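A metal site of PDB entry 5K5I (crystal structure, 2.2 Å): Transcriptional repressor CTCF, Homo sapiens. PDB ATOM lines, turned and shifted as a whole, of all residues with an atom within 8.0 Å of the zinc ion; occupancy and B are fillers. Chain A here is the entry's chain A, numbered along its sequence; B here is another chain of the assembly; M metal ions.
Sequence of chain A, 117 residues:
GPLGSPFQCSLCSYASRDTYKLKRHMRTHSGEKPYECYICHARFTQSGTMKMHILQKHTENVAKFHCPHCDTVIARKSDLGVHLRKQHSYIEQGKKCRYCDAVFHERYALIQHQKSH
O of His 25 is in hydrogen-bond range of OG1 of Thr 28 (2.7 Å).
A ring nitrogen (ND1) of His 25 sits at hydrogen-bond distance from OP1 of DA 9 of chain B (2.6 Å).
The side-chain sulfur of Cys 12 sits close to the backbone NH of Tyr 14.
SG of Cys 9 of chain A lies close to N of Leu 11 (3.5 Å).
The backbone carbonyl oxygen (O) of Tyr 14 sits at hydrogen-bond distance from the backbone NH (N) of Cys 9 of chain A, at 3.0 Å.
The side-chain sulfur (SG) of Cys 9 of chain A lies close to the side-chain sulfur (SD) of Met 26 (3.8 Å).
The zinc ion is bound by a ring nitrogen (NE2) of His 29, a ring nitrogen (NE2) of His 25, the side-chain sulfur of Cys 12 and the side-chain sulfur of Cys 9 of chain A.
Within 4 Å of the zinc ion: Cys 9 of chain A, Cys 12, His 25 and His 29.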
ATOM      1  N   GLN A   8      26.240  19.951  26.666  1.00  0.00           N
ATOM      2  CA  GLN A   8      26.609  21.362  26.719  1.00  0.00           C
ATOM      3  C   GLN A   8      28.008  21.550  26.132  1.00  0.00           C
ATOM      4  O   GLN A   8      28.917  20.771  26.409  1.00  0.00           O
ATOM      5  CB  GLN A   8      26.571  21.893  28.146  1.00  0.00           C
ATOM      6  CG  GLN A   8      26.880  23.377  28.290  1.00  0.00           C
ATOM      7  CD  GLN A   8      25.775  24.254  27.738  1.00  0.00           C
ATOM      8  OE1 GLN A   8      24.600  23.928  27.829  1.00  0.00           O
ATOM      9  NE2 GLN A   8      26.166  25.385  27.158  1.00  0.00           N
ATOM     10  N   CYS A   9      28.163  22.602  25.329  1.00  0.00           N
ATOM     11  CA  CYS A   9      29.474  22.924  24.767  1.00  0.00           C
ATOM     12  C   CYS A   9      30.377  23.522  25.836  1.00  0.00           C
ATOM     13  O   CYS A   9      29.928  24.194  26.769  1.00  0.00           O
ATOM     14  CB  CYS A   9      29.325  23.885  23.589  1.00  0.00           C
ATOM     15  SG  CYS A   9      30.900  24.346  22.818  1.00  0.00           S
ATOM     16  N   SER A  10      31.689  23.285  25.680  1.00  0.00           N
ATOM     17  CA  SER A  10      32.652  23.731  26.674  1.00  0.00           C
ATOM     18  C   SER A  10      33.091  25.174  26.447  1.00  0.00           C
ATOM     19  O   SER A  10      33.364  25.888  27.406  1.00  0.00           O
ATOM     20  CB  SER A  10      33.866  22.812  26.675  1.00  0.00           C
ATOM     21  OG  SER A  10      33.497  21.468  26.911  1.00  0.00           O
ATOM     22  N   LEU A  11      33.171  25.607  25.189  1.00  0.00           N
ATOM     23  CA  LEU A  11      33.714  26.921  24.855  1.00  0.00           C
ATOM     24  C   LEU A  11      32.651  27.963  24.556  1.00  0.00           C
ATOM     25  O   LEU A  11      32.995  29.135  24.372  1.00  0.00           O
ATOM     26  CB  LEU A  11      34.671  26.812  23.661  1.00  0.00           C
ATOM     27  CG  LEU A  11      35.857  25.857  23.848  1.00  0.00           C
ATOM     28  CD1 LEU A  11      36.763  25.886  22.633  1.00  0.00           C
ATOM     29  CD2 LEU A  11      36.618  26.189  25.116  1.00  0.00           C
ATOM     30  N   CYS A  12      31.376  27.589  24.515  1.00  0.00           N
ATOM     31  CA  CYS A  12      30.309  28.548  24.262  1.00  0.00           C
ATOM     32  C   CYS A  12      29.033  28.033  24.909  1.00  0.00           C
ATOM     33  O   CYS A  12      29.043  27.059  25.676  1.00  0.00           O
ATOM     34  CB  CYS A  12      30.135  28.793  22.756  1.00  0.00           C
ATOM     35  SG  CYS A  12      29.243  27.493  21.875  1.00  0.00           S
ATOM     36  N   SER A  13      27.910  28.693  24.603  1.00  0.00           N
ATOM     37  CA  SER A  13      26.628  28.399  25.234  1.00  0.00           C
ATOM     38  C   SER A  13      25.761  27.432  24.435  1.00  0.00           C
ATOM     39  O   SER A  13      24.618  27.178  24.829  1.00  0.00           O
ATOM     40  CB  SER A  13      25.859  29.701  25.470  1.00  0.00           C
ATOM     41  OG  SER A  13      26.626  30.608  26.239  1.00  0.00           O
ATOM     42  N   TYR A  14      26.271  26.898  23.321  1.00  0.00           N
ATOM     43  CA  TYR A  14      25.459  26.005  22.500  1.00  0.00           C
ATOM     44  C   TYR A  14      25.210  24.683  23.225  1.00  0.00           C
ATOM     45  O   TYR A  14      26.092  24.145  23.887  1.00  0.00           O
ATOM     46  CB  TYR A  14      26.146  25.745  21.164  1.00  0.00           C
ATOM     47  CG  TYR A  14      25.391  24.782  20.276  1.00  0.00           C
ATOM     48  CD1 TYR A  14      24.303  25.206  19.518  1.00  0.00           C
ATOM     49  CD2 TYR A  14      25.761  23.447  20.191  1.00  0.00           C
ATOM     50  CE1 TYR A  14      23.607  24.330  18.710  1.00  0.00           C
ATOM     51  CE2 TYR A  14      25.070  22.557  19.386  1.00  0.00           C
ATOM     52  CZ  TYR A  14      23.994  23.011  18.646  1.00  0.00           C
ATOM     53  OH  TYR A  14      23.307  22.130  17.835  1.00  0.00           O
ATOM     54  N   ALA A  15      23.998  24.174  23.078  1.00  0.00           N
ATOM     55  CA  ALA A  15      23.617  22.899  23.680  1.00  0.00           C
ATOM     56  C   ALA A  15      22.643  22.183  22.754  1.00  0.00           C
ATOM     57  O   ALA A  15      21.905  22.817  21.988  1.00  0.00           O
ATOM     58  CB  ALA A  15      22.984  23.103  25.066  1.00  0.00           C
ATOM     59  N   LEU A  22      26.485  18.241  18.627  1.00  0.00           N
ATOM     60  CA  LEU A  22      27.583  18.896  19.326  1.00  0.00           C
ATOM     61  C   LEU A  22      28.926  18.592  18.661  1.00  0.00           C
ATOM     62  O   LEU A  22      29.789  19.473  18.569  1.00  0.00           O
ATOM     63  CB  LEU A  22      27.608  18.483  20.796  1.00  0.00           C
ATOM     64  CG  LEU A  22      28.753  19.044  21.646  1.00  0.00           C
ATOM     65  CD1 LEU A  22      28.685  20.557  21.714  1.00  0.00           C
ATOM     66  CD2 LEU A  22      28.777  18.444  23.039  1.00  0.00           C
ATOM     67  N   HIS A  25      29.006  20.954  15.936  1.00  0.00           N
ATOM     68  CA  HIS A  25      29.203  22.318  16.414  1.00  0.00           C
ATOM     69  C   HIS A  25      30.644  22.574  16.837  1.00  0.00           C
ATOM     70  O   HIS A  25      31.135  23.697  16.708  1.00  0.00           O
ATOM     71  CB  HIS A  25      28.238  22.621  17.565  1.00  0.00           C
ATOM     72  CG  HIS A  25      28.586  23.873  18.324  1.00  0.00           C
ATOM     73  ND1 HIS A  25      28.408  25.131  17.801  1.00  0.00           N
ATOM     74  CD2 HIS A  25      29.104  24.045  19.558  1.00  0.00           C
ATOM     75  CE1 HIS A  25      28.794  26.027  18.691  1.00  0.00           C
ATOM     76  NE2 HIS A  25      29.226  25.404  19.768  1.00  0.00           N
ATOM     77  N   MET A  26      31.324  21.545  17.356  1.00  0.00           N
ATOM     78  CA  MET A  26      32.694  21.733  17.820  1.00  0.00           C
ATOM     79  C   MET A  26      33.655  22.081  16.688  1.00  0.00           C
ATOM     80  O   MET A  26      34.740  22.623  16.954  1.00  0.00           O
ATOM     81  CB  MET A  26      33.180  20.473  18.532  1.00  0.00           C
ATOM     82  CG  MET A  26      32.610  20.284  19.929  1.00  0.00           C
ATOM     83  SD  MET A  26      32.925  21.716  20.989  1.00  0.00           S
ATOM     84  CE  MET A  26      32.563  21.030  22.605  1.00  0.00           C
ATOM     85  N   ARG A  27      33.283  21.802  15.435  1.00  0.00           N
ATOM     86  CA  ARG A  27      34.137  22.176  14.305  1.00  0.00           C
ATOM     87  C   ARG A  27      34.257  23.688  14.148  1.00  0.00           C
ATOM     88  O   ARG A  27      35.226  24.165  13.553  1.00  0.00           O
ATOM     89  CB  ARG A  27      33.588  21.556  13.022  1.00  0.00           C
ATOM     90  CG  ARG A  27      33.436  20.046  13.076  1.00  0.00           C
ATOM     91  CD  ARG A  27      32.718  19.518  11.853  1.00  0.00           C
ATOM     92  NE  ARG A  27      32.399  18.096  11.981  1.00  0.00           N
ATOM     93  CZ  ARG A  27      31.635  17.416  11.129  1.00  0.00           C
ATOM     94  NH1 ARG A  27      31.102  18.027  10.077  1.00  0.00           N
ATOM     95  NH2 ARG A  27      31.402  16.125  11.329  1.00  0.00           N
ATOM     96  N   THR A  28      33.293  24.451  14.676  1.00  0.00           N
ATOM     97  CA  THR A  28      33.387  25.901  14.604  1.00  0.00           C
ATOM     98  C   THR A  28      34.521  26.439  15.469  1.00  0.00           C
ATOM     99  O   THR A  28      35.149  27.446  15.114  1.00  0.00           O
ATOM    100  CB  THR A  28      32.056  26.536  15.035  1.00  0.00           C
ATOM    101  OG1 THR A  28      31.800  26.249  16.411  1.00  0.00           O
ATOM    102  CG2 THR A  28      30.919  25.986  14.188  1.00  0.00           C
ATOM    103  N   HIS A  29      34.805  25.777  16.595  1.00  0.00           N
ATOM    104  CA  HIS A  29      35.888  26.173  17.479  1.00  0.00           C
ATOM    105  C   HIS A  29      37.231  25.590  17.059  1.00  0.00           C
ATOM    106  O   HIS A  29      38.244  26.301  17.052  1.00  0.00           O
ATOM    107  CB  HIS A  29      35.579  25.744  18.913  1.00  0.00           C
ATOM    108  CG  HIS A  29      34.319  26.328  19.479  1.00  0.00           C
ATOM    109  ND1 HIS A  29      34.188  27.665  19.766  1.00  0.00           N
ATOM    110  CD2 HIS A  29      33.140  25.757  19.805  1.00  0.00           C
ATOM    111  CE1 HIS A  29      32.976  27.901  20.239  1.00  0.00           C
ATOM    112  NE2 HIS A  29      32.323  26.746  20.277  1.00  0.00           N
ATOM    113  P    DA B   9      26.897  25.922  14.611  1.00  0.00           P
ATOM    114  OP1  DA B   9      27.241  26.455  15.945  1.00  0.00           O
ATOM    115  OP2  DA B   9      27.574  24.701  14.110  1.00  0.00           O
ATOM    116  O5'  DA B   9      25.323  25.661  14.565  1.00  0.00           O
ATOM    117  C5'  DA B   9      24.428  26.740  14.796  1.00  0.00           C
ATOM    118  C4'  DA B   9      23.005  26.350  14.436  1.00  0.00           C
ATOM    119  O4'  DA B   9      22.941  25.993  13.027  1.00  0.00           O
ATOM    120  C3'  DA B   9      22.447  25.157  15.215  1.00  0.00           C
ATOM    121  O3'  DA B   9      21.102  25.424  15.596  1.00  0.00           O
ATOM    122  C2'  DA B   9      22.533  24.015  14.210  1.00  0.00           C
ATOM    123  C1'  DA B   9      22.301  24.735  12.890  1.00  0.00           C
ATOM    124  N9   DA B   9      22.899  24.051  11.746  1.00  0.00           N
ATOM    125  C8   DA B   9      24.170  23.562  11.644  1.00  0.00           C
ATOM    126  N7   DA B   9      24.415  22.988  10.488  1.00  0.00           N
ATOM    127  C5   DA B   9      23.225  23.103   9.791  1.00  0.00           C
ATOM    128  C6   DA B   9      22.839  22.687   8.511  1.00  0.00           C
ATOM    129  N6   DA B   9      23.658  22.044   7.660  1.00  0.00           N
ATOM    130  N1   DA B   9      21.575  22.960   8.111  1.00  0.00           N
ATOM    131  C2   DA B   9      20.764  23.597   8.959  1.00  0.00           C
ATOM    132  N3   DA B   9      21.016  24.037  10.197  1.00  0.00           N
ATOM    133  C4   DA B   9      22.281  23.750  10.554  1.00  0.00           C
HETATM  134 ZN    ZN M   1      30.675  25.910  21.105  1.00  0.00          ZN
